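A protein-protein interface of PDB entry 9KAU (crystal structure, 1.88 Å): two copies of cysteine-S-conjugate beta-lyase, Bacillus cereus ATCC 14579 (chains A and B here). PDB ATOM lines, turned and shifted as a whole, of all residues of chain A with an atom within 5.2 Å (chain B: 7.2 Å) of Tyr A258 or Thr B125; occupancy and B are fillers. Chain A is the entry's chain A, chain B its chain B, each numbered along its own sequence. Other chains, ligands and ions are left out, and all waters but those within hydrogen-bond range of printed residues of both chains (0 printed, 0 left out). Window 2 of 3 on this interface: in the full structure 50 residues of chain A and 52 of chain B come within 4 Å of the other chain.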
ATOM      1  N   THR A 254       2.976  11.797  10.975  1.00  0.00           N
ATOM      2  CA  THR A 254       2.011  10.711  10.788  1.00  0.00           C
ATOM      3  C   THR A 254       2.539   9.377  11.334  1.00  0.00           C
ATOM      4  O   THR A 254       1.759   8.468  11.588  1.00  0.00           O
ATOM      5  CB  THR A 254       1.660  10.563   9.293  1.00  0.00           C
ATOM      6  OG1 THR A 254       2.866  10.356   8.544  1.00  0.00           O
ATOM      7  CG2 THR A 254       0.922  11.814   8.753  1.00  0.00           C
ATOM      8  N   ALA A 255       3.855   9.253  11.472  1.00  0.00           N
ATOM      9  CA  ALA A 255       4.454   8.091  12.084  1.00  0.00           C
ATOM     10  C   ALA A 255       4.090   7.993  13.550  1.00  0.00           C
ATOM     11  O   ALA A 255       3.765   6.911  14.055  1.00  0.00           O
ATOM     12  CB  ALA A 255       5.966   8.178  11.927  1.00  0.00           C
ATOM     13  N   ILE A 256       4.113   9.131  14.239  1.00  0.00           N
ATOM     14  CA  ILE A 256       3.804   9.193  15.660  1.00  0.00           C
ATOM     15  C   ILE A 256       2.328   8.937  15.907  1.00  0.00           C
ATOM     16  O   ILE A 256       1.952   8.297  16.898  1.00  0.00           O
ATOM     17  CB  ILE A 256       4.257  10.551  16.190  1.00  0.00           C
ATOM     18  CG1 ILE A 256       5.726  10.711  15.827  1.00  0.00           C
ATOM     19  CG2 ILE A 256       4.019  10.681  17.709  1.00  0.00           C
ATOM     20  CD1 ILE A 256       6.573   9.524  16.223  1.00  0.00           C
ATOM     21  N   GLN A 257       1.466   9.486  15.059  1.00  0.00           N
ATOM     22  CA  GLN A 257       0.053   9.161  15.161  1.00  0.00           C
ATOM     23  C   GLN A 257      -0.158   7.663  15.019  1.00  0.00           C
ATOM     24  O   GLN A 257      -1.004   7.083  15.703  1.00  0.00           O
ATOM     25  CB  GLN A 257      -0.759   9.894  14.104  1.00  0.00           C
ATOM     26  CG  GLN A 257      -0.732  11.382  14.151  1.00  0.00           C
ATOM     27  CD  GLN A 257      -1.566  11.929  13.038  1.00  0.00           C
ATOM     28  OE1 GLN A 257      -1.325  11.623  11.862  1.00  0.00           O
ATOM     29  NE2 GLN A 257      -2.575  12.722  13.389  1.00  0.00           N
ATOM     30  N   TYR A 258       0.537   7.037  14.075  1.00  0.00           N
ATOM     31  CA  TYR A 258       0.313   5.623  13.802  1.00  0.00           C
ATOM     32  C   TYR A 258       0.741   4.756  14.992  1.00  0.00           C
ATOM     33  O   TYR A 258      -0.002   3.874  15.422  1.00  0.00           O
ATOM     34  CB  TYR A 258       1.047   5.229  12.513  1.00  0.00           C
ATOM     35  CG  TYR A 258       0.750   3.837  12.083  1.00  0.00           C
ATOM     36  CD1 TYR A 258      -0.451   3.524  11.466  1.00  0.00           C
ATOM     37  CD2 TYR A 258       1.635   2.825  12.338  1.00  0.00           C
ATOM     38  CE1 TYR A 258      -0.751   2.238  11.094  1.00  0.00           C
ATOM     39  CE2 TYR A 258       1.346   1.525  11.977  1.00  0.00           C
ATOM     40  CZ  TYR A 258       0.157   1.242  11.350  1.00  0.00           C
ATOM     41  OH  TYR A 258      -0.123  -0.045  10.982  1.00  0.00           O
ATOM     42  N   ARG A 259       1.915   5.020  15.553  1.00  0.00           N
ATOM     43  CA  ARG A 259       2.397   4.344  16.746  1.00  0.00           C
ATOM     44  C   ARG A 259       1.542   4.602  17.996  1.00  0.00           C
ATOM     45  O   ARG A 259       1.820   3.991  19.034  1.00  0.00           O
ATOM     46  CB  ARG A 259       3.853   4.774  17.014  1.00  0.00           C
ATOM     47  CG  ARG A 259       3.943   6.247  17.460  1.00  0.00           C
ATOM     48  CD  ARG A 259       5.013   6.597  18.478  1.00  0.00           C
ATOM     49  NE  ARG A 259       6.350   6.608  17.929  1.00  0.00           N
ATOM     50  CZ  ARG A 259       7.396   7.165  18.521  1.00  0.00           C
ATOM     51  NH1 ARG A 259       7.262   7.749  19.701  1.00  0.00           N
ATOM     52  NH2 ARG A 259       8.577   7.121  17.941  1.00  0.00           N
ATOM     53  N   GLN A 260       0.614   5.558  17.980  1.00  0.00           N
ATOM     54  CA  GLN A 260      -0.304   5.740  19.104  1.00  0.00           C
ATOM     55  C   GLN A 260      -1.746   5.425  18.711  1.00  0.00           C
ATOM     56  O   GLN A 260      -2.677   5.955  19.331  1.00  0.00           O
ATOM     57  CB  GLN A 260      -0.190   7.134  19.729  1.00  0.00           C
ATOM     58  CG  GLN A 260       1.243   7.566  20.181  1.00  0.00           C
ATOM     59  CD  GLN A 260       1.420   9.090  20.325  1.00  0.00           C
ATOM     60  OE1 GLN A 260       0.449   9.831  20.210  1.00  0.00           O
ATOM     61  NE2 GLN A 260       2.652   9.553  20.557  1.00  0.00           N
ATOM     62  N   GLY A 261      -1.937   4.650  17.627  1.00  0.00           N
ATOM     63  CA  GLY A 261      -3.198   4.025  17.245  1.00  0.00           C
ATOM     64  C   GLY A 261      -4.224   4.891  16.544  1.00  0.00           C
ATOM     65  O   GLY A 261      -5.328   4.407  16.256  1.00  0.00           O
ATOM     66  N   PHE A 262      -3.893   6.146  16.229  1.00  0.00           N
ATOM     67  CA  PHE A 262      -4.803   7.074  15.510  1.00  0.00           C
ATOM     68  C   PHE A 262      -4.960   6.731  14.039  1.00  0.00           C
ATOM     69  O   PHE A 262      -3.911   6.665  13.381  1.00  0.00           O
ATOM     70  CB  PHE A 262      -4.294   8.508  15.548  1.00  0.00           C
ATOM     71  CG  PHE A 262      -5.188   9.522  14.892  1.00  0.00           C
ATOM     72  CD1 PHE A 262      -6.349   9.940  15.508  1.00  0.00           C
ATOM     73  CD2 PHE A 262      -4.852  10.067  13.667  1.00  0.00           C
ATOM     74  CE1 PHE A 262      -7.161  10.882  14.906  1.00  0.00           C
ATOM     75  CE2 PHE A 262      -5.669  10.999  13.062  1.00  0.00           C
ATOM     76  CZ  PHE A 262      -6.814  11.408  13.689  1.00  0.00           C
ATOM     77  N   HIS A 263      -6.214   6.577  13.573  1.00  0.00           N
ATOM     78  CA  HIS A 263      -6.496   6.215  12.183  1.00  0.00           C
ATOM     79  C   HIS A 263      -7.531   7.139  11.558  1.00  0.00           C
ATOM     80  O   HIS A 263      -8.223   6.739  10.613  1.00  0.00           O
ATOM     81  CB  HIS A 263      -6.951   4.755  12.062  1.00  0.00           C
ATOM     82  CG  HIS A 263      -5.960   3.777  12.610  1.00  0.00           C
ATOM     83  ND1 HIS A 263      -4.603   4.031  12.632  1.00  0.00           N
ATOM     84  CD2 HIS A 263      -6.123   2.559  13.178  1.00  0.00           C
ATOM     85  CE1 HIS A 263      -3.974   3.012  13.188  1.00  0.00           C
ATOM     86  NE2 HIS A 263      -4.873   2.103  13.523  1.00  0.00           N
ATOM     87  N   VAL B  92      -7.246   0.309  19.751  1.00  0.00           N
ATOM     88  CA  VAL B  92      -5.897   0.381  19.192  1.00  0.00           C
ATOM     89  C   VAL B  92      -5.031   1.414  19.894  1.00  0.00           C
ATOM     90  O   VAL B  92      -3.891   1.078  20.266  1.00  0.00           O
ATOM     91  CB  VAL B  92      -5.978   0.572  17.661  1.00  0.00           C
ATOM     92  CG1 VAL B  92      -4.675   0.154  17.006  1.00  0.00           C
ATOM     93  CG2 VAL B  92      -7.124  -0.251  17.090  1.00  0.00           C
ATOM     94  N   SER B  96      -1.504   0.637  22.268  1.00  0.00           N
ATOM     95  CA  SER B  96      -0.211   1.351  22.124  1.00  0.00           C
ATOM     96  C   SER B  96       0.199   1.963  23.449  1.00  0.00           C
ATOM     97  O   SER B  96       1.338   1.840  23.773  1.00  0.00           O
ATOM     98  CB  SER B  96      -0.299   2.382  21.075  1.00  0.00           C
ATOM     99  OG  SER B  96       0.740   3.317  21.238  1.00  0.00           O
ATOM    100  N   PRO B 117      -3.784  -7.894  13.143  1.00  0.00           N
ATOM    101  CA  PRO B 117      -2.473  -7.328  12.783  1.00  0.00           C
ATOM    102  C   PRO B 117      -2.070  -6.123  13.621  1.00  0.00           C
ATOM    103  O   PRO B 117      -0.873  -5.980  13.918  1.00  0.00           O
ATOM    104  CB  PRO B 117      -2.645  -6.958  11.306  1.00  0.00           C
ATOM    105  CG  PRO B 117      -3.733  -7.848  10.800  1.00  0.00           C
ATOM    106  CD  PRO B 117      -4.627  -8.157  11.959  1.00  0.00           C
ATOM    107  N   PRO B 118      -2.991  -5.248  14.055  1.00  0.00           N
ATOM    108  CA  PRO B 118      -2.540  -4.113  14.880  1.00  0.00           C
ATOM    109  C   PRO B 118      -1.745  -4.512  16.096  1.00  0.00           C
ATOM    110  O   PRO B 118      -0.818  -3.790  16.491  1.00  0.00           O
ATOM    111  CB  PRO B 118      -3.856  -3.439  15.275  1.00  0.00           C
ATOM    112  CG  PRO B 118      -4.701  -3.667  14.118  1.00  0.00           C
ATOM    113  CD  PRO B 118      -4.404  -5.073  13.678  1.00  0.00           C
ATOM    114  N   PHE B 120       0.485  -6.631  15.947  1.00  0.00           N
ATOM    115  CA  PHE B 120       1.818  -6.741  15.333  1.00  0.00           C
ATOM    116  C   PHE B 120       2.363  -5.355  15.070  1.00  0.00           C
ATOM    117  O   PHE B 120       3.430  -5.148  15.511  1.00  0.00           O
ATOM    118  CB  PHE B 120       1.770  -7.618  14.078  1.00  0.00           C
ATOM    119  CG  PHE B 120       1.486  -9.088  14.194  1.00  0.00           C
ATOM    120  CD1 PHE B 120       2.475  -9.974  14.564  1.00  0.00           C
ATOM    121  CD2 PHE B 120       0.256  -9.590  13.825  1.00  0.00           C
ATOM    122  CE1 PHE B 120       2.220 -11.332  14.621  1.00  0.00           C
ATOM    123  CE2 PHE B 120       0.004 -10.945  13.874  1.00  0.00           C
ATOM    124  CZ  PHE B 120       0.982 -11.814  14.279  1.00  0.00           C
ATOM    125  N   GLU B 121       1.590  -4.448  14.507  1.00  0.00           N
ATOM    126  CA  GLU B 121       2.140  -3.152  14.134  1.00  0.00           C
ATOM    127  C   GLU B 121       2.401  -2.279  15.369  1.00  0.00           C
ATOM    128  O   GLU B 121       3.445  -1.614  15.441  1.00  0.00           O
ATOM    129  CB  GLU B 121       1.206  -2.451  13.135  1.00  0.00           C
ATOM    130  CG  GLU B 121       1.239  -3.003  11.705  1.00  0.00           C
ATOM    131  CD  GLU B 121       2.612  -2.879  11.055  1.00  0.00           C
ATOM    132  OE1 GLU B 121       3.203  -1.788  11.158  1.00  0.00           O
ATOM    133  OE2 GLU B 121       3.088  -3.850  10.419  1.00  0.00           O
ATOM    134  N   MET B 122       1.534  -2.352  16.391  1.00  0.00           N
ATOM    135  CA  MET B 122       1.639  -1.423  17.520  1.00  0.00           C
ATOM    136  C   MET B 122       2.828  -1.746  18.416  1.00  0.00           C
ATOM    137  O   MET B 122       3.521  -0.848  18.897  1.00  0.00           O
ATOM    138  CB  MET B 122       0.335  -1.420  18.332  1.00  0.00           C
ATOM    139  CG  MET B 122      -0.939  -0.915  17.637  1.00  0.00           C
ATOM    140  SD  MET B 122      -0.644   0.446  16.468  1.00  0.00           S
ATOM    141  CE  MET B 122      -0.232   1.703  17.632  1.00  0.00           C
ATOM    142  N   VAL B 123       3.101  -3.016  18.617  1.00  0.00           N
ATOM    143  CA  VAL B 123       4.339  -3.412  19.270  1.00  0.00           C
ATOM    144  C   VAL B 123       5.529  -2.962  18.433  1.00  0.00           C
ATOM    145  O   VAL B 123       6.492  -2.371  18.940  1.00  0.00           O
ATOM    146  CB  VAL B 123       4.352  -4.940  19.446  1.00  0.00           C
ATOM    147  CG1 VAL B 123       5.689  -5.405  19.953  1.00  0.00           C
ATOM    148  CG2 VAL B 123       3.202  -5.372  20.303  1.00  0.00           C
ATOM    149  N   THR B 125       5.873  -0.819  15.619  1.00  0.00           N
ATOM    150  CA  THR B 125       5.996   0.610  15.248  1.00  0.00           C
ATOM    151  C   THR B 125       6.541   1.397  16.423  1.00  0.00           C
ATOM    152  O   THR B 125       7.242   2.379  16.171  1.00  0.00           O
ATOM    153  CB  THR B 125       4.703   1.178  14.672  1.00  0.00           C
ATOM    154  OG1 THR B 125       3.613   0.972  15.566  1.00  0.00           O
ATOM    155  CG2 THR B 125       4.408   0.642  13.291  1.00  0.00           C
ATOM    156  N   ASN B 126       6.299   0.924  17.633  1.00  0.00           N
ATOM    157  CA  ASN B 126       6.750   1.621  18.830  1.00  0.00           C
ATOM    158  C   ASN B 126       8.085   1.107  19.332  1.00  0.00           C
ATOM    159  O   ASN B 126       8.416   1.308  20.502  1.00  0.00           O
ATOM    160  CB  ASN B 126       5.716   1.512  19.941  1.00  0.00           C
ATOM    161  CG  ASN B 126       4.655   2.569  19.862  1.00  0.00           C
ATOM    162  OD1 ASN B 126       4.877   3.720  20.215  1.00  0.00           O
ATOM    163  ND2 ASN B 126       3.480   2.181  19.399  1.00  0.00           N
ATOM    164  N   ARG B 128       9.079  -1.885  20.108  1.00  0.00           N
ATOM    165  CA  ARG B 128       9.201  -3.011  21.016  1.00  0.00           C
ATOM    166  C   ARG B 128       9.463  -4.296  20.241  1.00  0.00           C
ATOM    167  O   ARG B 128       9.321  -4.360  19.014  1.00  0.00           O
ATOM    168  CB  ARG B 128       7.962  -3.161  21.875  1.00  0.00           C
ATOM    169  CG  ARG B 128       8.148  -2.481  23.186  1.00  0.00           C
ATOM    170  CD  ARG B 128       7.875  -1.015  23.024  1.00  0.00           C
ATOM    171  NE  ARG B 128       7.747  -0.364  24.309  1.00  0.00           N
ATOM    172  CZ  ARG B 128       8.321   0.786  24.572  1.00  0.00           C
ATOM    173  NH1 ARG B 128       9.033   1.373  23.633  1.00  0.00           N
ATOM    174  NH2 ARG B 128       8.177   1.339  25.761  1.00  0.00           N
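Ile A256 touches none of the printed residues of chain B. Tyr A258 touches just these residues of chain B: Glu B121 (3.3 Å), Met B122 (3.1 Å) and Thr B125 (3.4 Å). Printed residues of chain B within 4 Å of Gly A261: Met B122 (3.4 Å). Printed residues of chain A within 4 Å of Val B92: His A263. Of the printed residues of chain A, Glu B121 touches Tyr A258. Printed residues of chain A within 4 Å of Met B122: Tyr A258, Arg A259, Gln A260 and Gly A261. Printed residues of chain A within 4 Å of Thr B125: Tyr A258 (3.4 Å) and Arg A259 (3.8 Å). Of the printed residues of chain A, Asn B126 touches Arg A259. Arg B128 touches none of the printed residues of chain A. The nearest printed residue of chain A that does not touch Ser B96 is Gly A261 (4.4 Å).
Hydrophobic or aromatic side chains of chain A within 4 Å of the printed part of chain B: Tyr A258 and His A263. Printed residues of chain B that touch a printed residue of chain A: Val B92, Ser B96, Glu B121, Met B122, Thr B125 and Asn B126. Hydrophobic or aromatic side chains of chain B that line the printed part of chain A: Val B92 and Met B122. Among the printed residues, no Asp or Glu carboxylate lies within 4 Å of a Lys or Arg side-chain nitrogen of the other chain.
The side-chain hydroxyl (OG) of Ser B96 lies within hydrogen-bond range of the side-chain amide nitrogen (ND2) of Asn B126 (3.5 Å). The backbone carbonyl oxygen of Glu B121 lies within hydrogen-bond range of the side-chain hydroxyl of Thr B125 (2.6 Å). The backbone carbonyl oxygen (O) of Asn B126 lies within hydrogen-bond range of the guanidinium group (NH1) of Arg B128, at 3.2 Å. The backbone carbonyl oxygen (O) of Met B122 sits at hydrogen-bond distance from the side-chain amide nitrogen (ND2) of Asn B126 (3.1 Å).
CG of Glu B121 touches OH of Tyr A258 (3.3 Å). Tyr A258 touches Thr B125 (CE2 to CG2, 3.4 Å). Arg A259 touches Met B122 (O to CE, 3.4 Å). Arg A259 touches Thr B125 (CA to OG1, 3.8 Å). Gln A260 touches Ser B96. N of Gln A260 touches CE of Met B122 (3.96 Å). Met B122 touches Gly A261. NE2 of His A263 touches CG1 of Val B92, 3.996 Å away.
No position is printed for both chains. Of the 11 pairs that touch across the chains among the printed residues, none has its exchanged pair printed and touching as well.
SD of Met B122 lies close to O of Tyr A258 (3.6 Å). The backbone carbonyl oxygen of Arg A259 is in hydrogen-bond range of the side-chain hydroxyl of Ser B96 (2.5 Å). ND2 of Asn B126 sits at hydrogen-bond distance from O of Arg A259 (2.5 Å).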
